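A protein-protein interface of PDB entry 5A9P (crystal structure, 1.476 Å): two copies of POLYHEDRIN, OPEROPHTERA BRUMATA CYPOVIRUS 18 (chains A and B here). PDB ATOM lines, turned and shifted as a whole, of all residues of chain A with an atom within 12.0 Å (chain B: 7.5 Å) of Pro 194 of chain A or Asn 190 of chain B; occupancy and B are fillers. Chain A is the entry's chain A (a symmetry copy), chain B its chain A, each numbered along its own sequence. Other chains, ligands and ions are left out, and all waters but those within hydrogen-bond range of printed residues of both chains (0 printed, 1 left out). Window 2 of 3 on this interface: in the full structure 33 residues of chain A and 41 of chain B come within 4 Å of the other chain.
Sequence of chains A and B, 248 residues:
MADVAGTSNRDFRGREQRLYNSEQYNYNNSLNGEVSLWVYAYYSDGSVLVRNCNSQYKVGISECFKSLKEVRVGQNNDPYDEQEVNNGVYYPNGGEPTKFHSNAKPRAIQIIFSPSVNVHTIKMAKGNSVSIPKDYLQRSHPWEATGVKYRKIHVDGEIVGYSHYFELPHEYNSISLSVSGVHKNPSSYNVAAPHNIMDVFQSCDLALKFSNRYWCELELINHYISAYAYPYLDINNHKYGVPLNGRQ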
ATOM      1  N   TYR A  57       4.172  29.781  13.824  1.00  0.00           N
ATOM      2  CA  TYR A  57       3.481  28.520  13.490  1.00  0.00           C
ATOM      3  C   TYR A  57       2.577  27.948  14.583  1.00  0.00           C
ATOM      4  O   TYR A  57       1.436  27.568  14.318  1.00  0.00           O
ATOM      5  CB  TYR A  57       4.477  27.436  13.079  1.00  0.00           C
ATOM      6  CG  TYR A  57       5.455  27.846  12.002  1.00  0.00           C
ATOM      7  CD1 TYR A  57       5.017  28.222  10.748  1.00  0.00           C
ATOM      8  CD2 TYR A  57       6.819  27.833  12.243  1.00  0.00           C
ATOM      9  CE1 TYR A  57       5.907  28.589   9.758  1.00  0.00           C
ATOM     10  CE2 TYR A  57       7.726  28.192  11.265  1.00  0.00           C
ATOM     11  CZ  TYR A  57       7.263  28.564  10.016  1.00  0.00           C
ATOM     12  OH  TYR A  57       8.152  28.920   9.030  1.00  0.00           O
ATOM     13  N   ASN A 185      -3.854  29.402   9.504  1.00  0.00           N
ATOM     14  CA  ASN A 185      -3.358  29.082   8.180  1.00  0.00           C
ATOM     15  C   ASN A 185      -4.517  28.730   7.263  1.00  0.00           C
ATOM     16  O   ASN A 185      -4.886  27.557   7.141  1.00  0.00           O
ATOM     17  CB  ASN A 185      -2.361  27.932   8.200  1.00  0.00           C
ATOM     18  CG  ASN A 185      -1.813  27.642   6.825  1.00  0.00           C
ATOM     19  OD1 ASN A 185      -2.030  28.410   5.897  1.00  0.00           O
ATOM     20  ND2 ASN A 185      -1.107  26.539   6.682  1.00  0.00           N
ATOM     21  N   SER A 188      -3.868  26.036   1.985  1.00  0.00           N
ATOM     22  CA  SER A 188      -3.752  24.588   2.057  1.00  0.00           C
ATOM     23  C   SER A 188      -2.284  24.149   2.114  1.00  0.00           C
ATOM     24  O   SER A 188      -1.990  22.957   2.128  1.00  0.00           O
ATOM     25  CB  SER A 188      -4.481  23.928   0.883  1.00  0.00           C
ATOM     26  OG  SER A 188      -4.052  24.443  -0.363  1.00  0.00           O
ATOM     27  N   TYR A 189      -1.365  25.111   2.176  1.00  0.00           N
ATOM     28  CA  TYR A 189       0.052  24.800   2.336  1.00  0.00           C
ATOM     29  C   TYR A 189       0.337  24.442   3.793  1.00  0.00           C
ATOM     30  O   TYR A 189       0.219  25.277   4.690  1.00  0.00           O
ATOM     31  CB  TYR A 189       0.913  25.983   1.892  1.00  0.00           C
ATOM     32  CG  TYR A 189       2.412  25.773   2.002  1.00  0.00           C
ATOM     33  CD1 TYR A 189       3.089  26.051   3.184  1.00  0.00           C
ATOM     34  CD2 TYR A 189       3.150  25.327   0.915  1.00  0.00           C
ATOM     35  CE1 TYR A 189       4.460  25.872   3.288  1.00  0.00           C
ATOM     36  CE2 TYR A 189       4.525  25.144   1.006  1.00  0.00           C
ATOM     37  CZ  TYR A 189       5.173  25.427   2.196  1.00  0.00           C
ATOM     38  OH  TYR A 189       6.537  25.249   2.284  1.00  0.00           O
ATOM     39  N   ASN A 190       0.703  23.190   4.022  1.00  0.00           N
ATOM     40  CA  ASN A 190       0.986  22.716   5.368  1.00  0.00           C
ATOM     41  C   ASN A 190       2.369  23.194   5.794  1.00  0.00           C
ATOM     42  O   ASN A 190       3.368  22.788   5.208  1.00  0.00           O
ATOM     43  CB  ASN A 190       0.910  21.190   5.380  1.00  0.00           C
ATOM     44  CG  ASN A 190       0.923  20.606   6.780  1.00  0.00           C
ATOM     45  OD1 ASN A 190       1.489  21.184   7.715  1.00  0.00           O
ATOM     46  ND2 ASN A 190       0.304  19.437   6.929  1.00  0.00           N
ATOM     47  N   VAL A 191       2.437  24.066   6.800  1.00  0.00           N
ATOM     48  CA  VAL A 191       3.729  24.612   7.216  1.00  0.00           C
ATOM     49  C   VAL A 191       4.650  23.547   7.796  1.00  0.00           C
ATOM     50  O   VAL A 191       5.852  23.775   7.927  1.00  0.00           O
ATOM     51  CB  VAL A 191       3.602  25.753   8.253  1.00  0.00           C
ATOM     52  CG1 VAL A 191       2.842  26.928   7.666  1.00  0.00           C
ATOM     53  CG2 VAL A 191       2.957  25.256   9.552  1.00  0.00           C
ATOM     54  N   ALA A 192       4.084  22.394   8.150  1.00  0.00           N
ATOM     55  CA  ALA A 192       4.854  21.310   8.756  1.00  0.00           C
ATOM     56  C   ALA A 192       4.957  20.075   7.859  1.00  0.00           C
ATOM     57  O   ALA A 192       5.356  19.004   8.312  1.00  0.00           O
ATOM     58  CB  ALA A 192       4.271  20.937  10.110  1.00  0.00           C
ATOM     59  N   ALA A 193       4.605  20.221   6.587  1.00  0.00           N
ATOM     60  CA  ALA A 193       4.913  19.186   5.607  1.00  0.00           C
ATOM     61  C   ALA A 193       6.388  19.347   5.235  1.00  0.00           C
ATOM     62  O   ALA A 193       7.015  20.327   5.626  1.00  0.00           O
ATOM     63  CB  ALA A 193       4.007  19.304   4.398  1.00  0.00           C
ATOM     64  N   PRO A 194       6.960  18.378   4.510  1.00  0.00           N
ATOM     65  CA  PRO A 194       8.417  18.367   4.317  1.00  0.00           C
ATOM     66  C   PRO A 194       9.062  19.641   3.747  1.00  0.00           C
ATOM     67  O   PRO A 194      10.205  19.929   4.101  1.00  0.00           O
ATOM     68  CB  PRO A 194       8.621  17.175   3.382  1.00  0.00           C
ATOM     69  CG  PRO A 194       7.540  16.229   3.811  1.00  0.00           C
ATOM     70  CD  PRO A 194       6.346  17.118   4.046  1.00  0.00           C
ATOM     71  N   HIS A 195       8.371  20.396   2.900  1.00  0.00           N
ATOM     72  CA  HIS A 195       8.978  21.608   2.343  1.00  0.00           C
ATOM     73  C   HIS A 195       9.361  22.633   3.406  1.00  0.00           C
ATOM     74  O   HIS A 195      10.236  23.458   3.164  1.00  0.00           O
ATOM     75  CB  HIS A 195       8.057  22.294   1.338  1.00  0.00           C
ATOM     76  CG  HIS A 195       8.170  21.760  -0.055  1.00  0.00           C
ATOM     77  ND1 HIS A 195       7.952  22.544  -1.167  1.00  0.00           N
ATOM     78  CD2 HIS A 195       8.470  20.524  -0.517  1.00  0.00           C
ATOM     79  CE1 HIS A 195       8.112  21.812  -2.256  1.00  0.00           C
ATOM     80  NE2 HIS A 195       8.429  20.584  -1.889  1.00  0.00           N
ATOM     81  N   ASN A 196       8.707  22.609   4.565  1.00  0.00           N
ATOM     82  CA  ASN A 196       8.969  23.616   5.595  1.00  0.00           C
ATOM     83  C   ASN A 196       9.088  23.055   7.018  1.00  0.00           C
ATOM     84  O   ASN A 196       9.338  23.800   7.963  1.00  0.00           O
ATOM     85  CB  ASN A 196       7.883  24.693   5.544  1.00  0.00           C
ATOM     86  CG  ASN A 196       8.256  25.941   6.323  1.00  0.00           C
ATOM     87  OD1 ASN A 196       9.216  26.636   5.978  1.00  0.00           O
ATOM     88  ND2 ASN A 196       7.487  26.245   7.364  1.00  0.00           N
ATOM     89  N   ILE A 197       8.938  21.744   7.168  1.00  0.00           N
ATOM     90  CA  ILE A 197       8.945  21.104   8.484  1.00  0.00           C
ATOM     91  C   ILE A 197      10.135  21.484   9.381  1.00  0.00           C
ATOM     92  O   ILE A 197       9.954  21.709  10.574  1.00  0.00           O
ATOM     93  CB  ILE A 197       8.860  19.553   8.349  1.00  0.00           C
ATOM     94  CG1 ILE A 197       8.925  18.860   9.717  1.00  0.00           C
ATOM     95  CG2 ILE A 197       9.983  19.021   7.480  1.00  0.00           C
ATOM     96  CD1 ILE A 197       7.865  19.283  10.696  1.00  0.00           C
ATOM     97  N   MET A 198      11.350  21.548   8.847  1.00  0.00           N
ATOM     98  CA  MET A 198      12.484  21.807   9.732  1.00  0.00           C
ATOM     99  C   MET A 198      12.389  23.211  10.325  1.00  0.00           C
ATOM    100  O   MET A 198      12.857  23.453  11.439  1.00  0.00           O
ATOM    101  CB  MET A 198      13.827  21.596   9.034  1.00  0.00           C
ATOM    102  CG  MET A 198      15.027  21.650   9.983  1.00  0.00           C
ATOM    103  SD  MET A 198      14.918  20.509  11.389  1.00  0.00           S
ATOM    104  CE  MET A 198      14.650  18.965  10.543  1.00  0.00           C
ATOM    105  N   ASP A 199      11.746  24.127   9.604  1.00  0.00           N
ATOM    106  CA  ASP A 199      11.528  25.471  10.128  1.00  0.00           C
ATOM    107  C   ASP A 199      10.579  25.476  11.326  1.00  0.00           C
ATOM    108  O   ASP A 199      10.727  26.280  12.249  1.00  0.00           O
ATOM    109  CB  ASP A 199      11.000  26.399   9.033  1.00  0.00           C
ATOM    110  CG  ASP A 199      12.093  26.881   8.112  1.00  0.00           C
ATOM    111  OD1 ASP A 199      12.881  26.037   7.640  1.00  0.00           O
ATOM    112  OD2 ASP A 199      12.178  28.103   7.870  1.00  0.00           O
ATOM    113  N   VAL A 200       9.602  24.579  11.319  1.00  0.00           N
ATOM    114  CA  VAL A 200       8.714  24.465  12.470  1.00  0.00           C
ATOM    115  C   VAL A 200       9.493  23.899  13.658  1.00  0.00           C
ATOM    116  O   VAL A 200       9.301  24.333  14.784  1.00  0.00           O
ATOM    117  CB  VAL A 200       7.472  23.611  12.160  1.00  0.00           C
ATOM    118  CG1 VAL A 200       6.514  23.608  13.348  1.00  0.00           C
ATOM    119  CG2 VAL A 200       6.773  24.141  10.916  1.00  0.00           C
ATOM    120  N   PHE A 201      10.389  22.946  13.412  1.00  0.00           N
ATOM    121  CA  PHE A 201      11.266  22.475  14.484  1.00  0.00           C
ATOM    122  C   PHE A 201      12.120  23.623  15.033  1.00  0.00           C
ATOM    123  O   PHE A 201      12.277  23.767  16.242  1.00  0.00           O
ATOM    124  CB  PHE A 201      12.158  21.323  14.009  1.00  0.00           C
ATOM    125  CG  PHE A 201      11.500  19.978  14.099  1.00  0.00           C
ATOM    126  CD1 PHE A 201      11.223  19.417  15.337  1.00  0.00           C
ATOM    127  CD2 PHE A 201      11.148  19.283  12.957  1.00  0.00           C
ATOM    128  CE1 PHE A 201      10.616  18.191  15.433  1.00  0.00           C
ATOM    129  CE2 PHE A 201      10.530  18.049  13.048  1.00  0.00           C
ATOM    130  CZ  PHE A 201      10.255  17.509  14.286  1.00  0.00           C
ATOM    131  N   GLN A 202      12.666  24.448  14.148  1.00  0.00           N
ATOM    132  CA  GLN A 202      13.443  25.598  14.594  1.00  0.00           C
ATOM    133  C   GLN A 202      12.590  26.594  15.383  1.00  0.00           C
ATOM    134  O   GLN A 202      13.085  27.227  16.312  1.00  0.00           O
ATOM    135  CB  GLN A 202      14.104  26.297  13.408  1.00  0.00           C
ATOM    136  CG  GLN A 202      15.221  25.487  12.769  1.00  0.00           C
ATOM    137  CD  GLN A 202      16.083  26.327  11.851  1.00  0.00           C
ATOM    138  OE1 GLN A 202      15.804  26.464  10.661  1.00  0.00           O
ATOM    139  NE2 GLN A 202      17.145  26.896  12.405  1.00  0.00           N
ATOM    140  N   LEU B  31      24.574  12.563   9.298  1.00  0.00           N
ATOM    141  CA  LEU B  31      23.267  12.821   9.890  1.00  0.00           C
ATOM    142  C   LEU B  31      23.130  12.111  11.231  1.00  0.00           C
ATOM    143  O   LEU B  31      22.232  12.420  12.009  1.00  0.00           O
ATOM    144  CB  LEU B  31      22.143  12.404   8.941  1.00  0.00           C
ATOM    145  CG  LEU B  31      22.146  13.097   7.578  1.00  0.00           C
ATOM    146  CD1 LEU B  31      21.037  12.534   6.704  1.00  0.00           C
ATOM    147  CD2 LEU B  31      21.992  14.605   7.715  1.00  0.00           C
ATOM    148  N   ASN B 185      23.055  18.947   6.000  1.00  0.00           N
ATOM    149  CA  ASN B 185      22.506  17.817   5.278  1.00  0.00           C
ATOM    150  C   ASN B 185      22.615  18.055   3.781  1.00  0.00           C
ATOM    151  O   ASN B 185      21.688  18.588   3.162  1.00  0.00           O
ATOM    152  CB  ASN B 185      21.053  17.550   5.643  1.00  0.00           C
ATOM    153  CG  ASN B 185      20.508  16.340   4.925  1.00  0.00           C
ATOM    154  OD1 ASN B 185      21.259  15.598   4.305  1.00  0.00           O
ATOM    155  ND2 ASN B 185      19.208  16.135   4.998  1.00  0.00           N
ATOM    156  N   SER B 187      22.649  15.826   1.524  1.00  0.00           N
ATOM    157  CA  SER B 187      21.821  14.861   0.822  1.00  0.00           C
ATOM    158  C   SER B 187      20.466  15.506   0.545  1.00  0.00           C
ATOM    159  O   SER B 187      20.153  16.558   1.099  1.00  0.00           O
ATOM    160  CB  SER B 187      21.647  13.593   1.667  1.00  0.00           C
ATOM    161  OG  SER B 187      20.528  13.694   2.530  1.00  0.00           O
ATOM    162  N   SER B 188      19.668  14.869  -0.305  1.00  0.00           N
ATOM    163  CA  SER B 188      18.303  15.307  -0.542  1.00  0.00           C
ATOM    164  C   SER B 188      17.309  14.530   0.331  1.00  0.00           C
ATOM    165  O   SER B 188      16.102  14.730   0.231  1.00  0.00           O
ATOM    166  CB  SER B 188      17.945  15.187  -2.026  1.00  0.00           C
ATOM    167  OG  SER B 188      18.189  13.886  -2.525  1.00  0.00           O
ATOM    168  N   TYR B 189      17.819  13.665   1.206  1.00  0.00           N
ATOM    169  CA  TYR B 189      16.967  12.950   2.153  1.00  0.00           C
ATOM    170  C   TYR B 189      16.587  13.881   3.302  1.00  0.00           C
ATOM    171  O   TYR B 189      17.435  14.307   4.087  1.00  0.00           O
ATOM    172  CB  TYR B 189      17.682  11.704   2.680  1.00  0.00           C
ATOM    173  CG  TYR B 189      16.888  10.871   3.668  1.00  0.00           C
ATOM    174  CD1 TYR B 189      16.917  11.152   5.029  1.00  0.00           C
ATOM    175  CD2 TYR B 189      16.135   9.785   3.241  1.00  0.00           C
ATOM    176  CE1 TYR B 189      16.204  10.387   5.939  1.00  0.00           C
ATOM    177  CE2 TYR B 189      15.416   9.010   4.143  1.00  0.00           C
ATOM    178  CZ  TYR B 189      15.463   9.315   5.493  1.00  0.00           C
ATOM    179  OH  TYR B 189      14.752   8.543   6.387  1.00  0.00           O
ATOM    180  N   ASN B 190      15.305  14.200   3.390  1.00  0.00           N
ATOM    181  CA  ASN B 190      14.814  15.093   4.428  1.00  0.00           C
ATOM    182  C   ASN B 190      14.709  14.331   5.744  1.00  0.00           C
ATOM    183  O   ASN B 190      13.909  13.407   5.859  1.00  0.00           O
ATOM    184  CB  ASN B 190      13.451  15.640   4.006  1.00  0.00           C
ATOM    185  CG  ASN B 190      12.972  16.781   4.884  1.00  0.00           C
ATOM    186  OD1 ASN B 190      13.311  16.869   6.070  1.00  0.00           O
ATOM    187  ND2 ASN B 190      12.160  17.662   4.302  1.00  0.00           N
ATOM    188  N   VAL B 191      15.520  14.699   6.736  1.00  0.00           N
ATOM    189  CA  VAL B 191      15.514  13.967   8.003  1.00  0.00           C
ATOM    190  C   VAL B 191      14.193  14.107   8.747  1.00  0.00           C
ATOM    191  O   VAL B 191      13.920  13.340   9.671  1.00  0.00           O
ATOM    192  CB  VAL B 191      16.651  14.397   8.960  1.00  0.00           C
ATOM    193  CG1 VAL B 191      18.008  14.112   8.341  1.00  0.00           C
ATOM    194  CG2 VAL B 191      16.513  15.869   9.364  1.00  0.00           C
ATOM    195  N   ALA B 192      13.384  15.089   8.353  1.00  0.00           N
ATOM    196  CA  ALA B 192      12.107  15.351   9.014  1.00  0.00           C
ATOM    197  C   ALA B 192      10.900  15.063   8.120  1.00  0.00           C
ATOM    198  O   ALA B 192       9.779  15.457   8.436  1.00  0.00           O
ATOM    199  CB  ALA B 192      12.059  16.781   9.529  1.00  0.00           C
ATOM    200  N   ALA B 193      11.122  14.371   7.008  1.00  0.00           N
ATOM    201  CA  ALA B 193      10.010  13.828   6.236  1.00  0.00           C
ATOM    202  C   ALA B 193       9.544  12.560   6.952  1.00  0.00           C
ATOM    203  O   ALA B 193      10.202  12.106   7.883  1.00  0.00           O
ATOM    204  CB  ALA B 193      10.434  13.551   4.807  1.00  0.00           C
ATOM    205  N   PRO B 194       8.397  12.000   6.550  1.00  0.00           N
ATOM    206  CA  PRO B 194       7.790  10.921   7.342  1.00  0.00           C
ATOM    207  C   PRO B 194       8.669   9.700   7.661  1.00  0.00           C
ATOM    208  O   PRO B 194       8.484   9.106   8.723  1.00  0.00           O
ATOM    209  CB  PRO B 194       6.579  10.527   6.496  1.00  0.00           C
ATOM    210  CG  PRO B 194       6.170  11.830   5.876  1.00  0.00           C
ATOM    211  CD  PRO B 194       7.476  12.485   5.504  1.00  0.00           C
ATOM    212  N   HIS B 195       9.602   9.327   6.793  1.00  0.00           N
ATOM    213  CA  HIS B 195      10.440   8.159   7.082  1.00  0.00           C
ATOM    214  C   HIS B 195      11.266   8.311   8.356  1.00  0.00           C
ATOM    215  O   HIS B 195      11.655   7.310   8.948  1.00  0.00           O
ATOM    216  CB  HIS B 195      11.397   7.849   5.935  1.00  0.00           C
ATOM    217  CG  HIS B 195      10.805   6.990   4.863  1.00  0.00           C
ATOM    218  ND1 HIS B 195      11.562   6.116   4.113  1.00  0.00           N
ATOM    219  CD2 HIS B 195       9.535   6.872   4.410  1.00  0.00           C
ATOM    220  CE1 HIS B 195      10.783   5.499   3.243  1.00  0.00           C
ATOM    221  NE2 HIS B 195       9.548   5.937   3.404  1.00  0.00           N
ATOM    222  N   ASN B 196      11.558   9.542   8.771  1.00  0.00           N
ATOM    223  CA  ASN B 196      12.415   9.756   9.938  1.00  0.00           C
ATOM    224  C   ASN B 196      11.914  10.837  10.906  1.00  0.00           C
ATOM    225  O   ASN B 196      12.533  11.084  11.938  1.00  0.00           O
ATOM    226  CB  ASN B 196      13.836  10.085   9.475  1.00  0.00           C
ATOM    227  CG  ASN B 196      14.858   9.976  10.592  1.00  0.00           C
ATOM    228  OD1 ASN B 196      15.090   8.891  11.131  1.00  0.00           O
ATOM    229  ND2 ASN B 196      15.491  11.095  10.929  1.00  0.00           N
ATOM    230  N   ILE B 197      10.784  11.457  10.590  1.00  0.00           N
ATOM    231  CA  ILE B 197      10.252  12.562  11.388  1.00  0.00           C
ATOM    232  C   ILE B 197      10.155  12.282  12.897  1.00  0.00           C
ATOM    233  O   ILE B 197      10.485  13.147  13.703  1.00  0.00           O
ATOM    234  CB  ILE B 197       8.864  13.022  10.847  1.00  0.00           C
ATOM    235  CG1 ILE B 197       8.262  14.142  11.708  1.00  0.00           C
ATOM    236  CG2 ILE B 197       7.887  11.864  10.804  1.00  0.00           C
ATOM    237  CD1 ILE B 197       9.119  15.370  11.844  1.00  0.00           C
ATOM    238  N   VAL B 200      13.280  12.968  14.737  1.00  0.00           N
ATOM    239  CA  VAL B 200      13.584  14.375  14.973  1.00  0.00           C
ATOM    240  C   VAL B 200      12.801  14.865  16.193  1.00  0.00           C
ATOM    241  O   VAL B 200      13.323  15.625  16.995  1.00  0.00           O
ATOM    242  CB  VAL B 200      13.294  15.246  13.738  1.00  0.00           C
ATOM    243  CG1 VAL B 200      13.728  16.687  13.985  1.00  0.00           C
ATOM    244  CG2 VAL B 200      14.007  14.676  12.520  1.00  0.00           C
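Pro 194 of chain A touches Asn 190 of chain B, but with the chains exchanged Asn 190 of chain A does not touch Pro 194 of chain B (9.7 Å).
Ile 197 of chain A touches Ala 192 of chain B, but with the chains exchanged Ala 192 of chain A does not touch Ile 197 of chain B (6.3 Å).
Of the 6 pairs that touch across the chains among the printed residues, none has its exchanged pair printed and touching as well.
Ala 192 of chain B touches Ile 197 of chain A (CB to CG2, 3.7 Å).
CE of Met 198 of chain A touches CG2 of Val 191 of chain B, at 3.8 Å.
Met 198 of chain A touches Ala 192 of chain B.
Phe 201 of chain A touches Ile 197 of chain B.
Phe 201 of chain A touches Val 200 of chain B.
The side-chain amide nitrogen of Asn 190 of chain B sits at hydrogen-bond distance from the backbone carbonyl oxygen of Pro 194 of chain A.
Of the printed residues of chain B, Ile 197 of chain A touches Ala 192 (3.7 Å).
Of the printed residues of chain B, Met 198 of chain A touches Val 191 (3.8 Å) and Ala 192 (3.5 Å).
Asp 199 of chain A touches none of the printed residues of chain B.
Printed residues of chain B within 4 Å of Phe 201 of chain A: Ile 197 (3.3 Å) and Val 200 (3.6 Å).
No residue of chain A comes within 4 Å of Ser 187 of chain B.
No residue of chain A comes within 4 Å of Ser 188 of chain B.
Tyr 189 of chain B touches none of the printed residues of chain A.
Asn 190 of chain B touches one residue of chain A.
Of chain A, only Met 198 comes within 4 Å of Val 191 of chain B.
No residue of chain A comes within 4 Å of Ala 193 of chain B.
No residue of chain A comes within 4 Å of Asn 196 of chain B.
Of the printed residues of chain A, Ile 197 of chain B touches Phe 201.
Of the printed residues of chain A, Val 200 of chain B touches Phe 201.
The nearest residue of chain A that does not touch Asn 190 of chain B is Ile 197 of chain A (4.1 Å).
The nearest printed residue of chain A that does not touch Val 200 of chain B is Met 198 of chain A (4.2 Å).
The backbone carbonyl oxygen of Val 191 of chain B lies within hydrogen-bond range of the side-chain amide nitrogen of Asn 196 of chain B, at 3.0 Å.
N of Ala 193 of chain B is in hydrogen-bond range of OD1 of Asn 190 of chain B (3.5 Å).
The backbone NH (N) of Ala 192 of chain B lies within hydrogen-bond range of the side-chain amide oxygen (OD1) of Asn 190 of chain B, at 2.9 Å.
Hydrophobic or aromatic side chains of chain A within 4 Å of the printed part of chain B: Pro 194, Ile 197, Met 198 and Phe 201.
Among the printed residues, no Asp or Glu carboxylate lies within 4 Å of a Lys or Arg side-chain nitrogen of the other chain.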
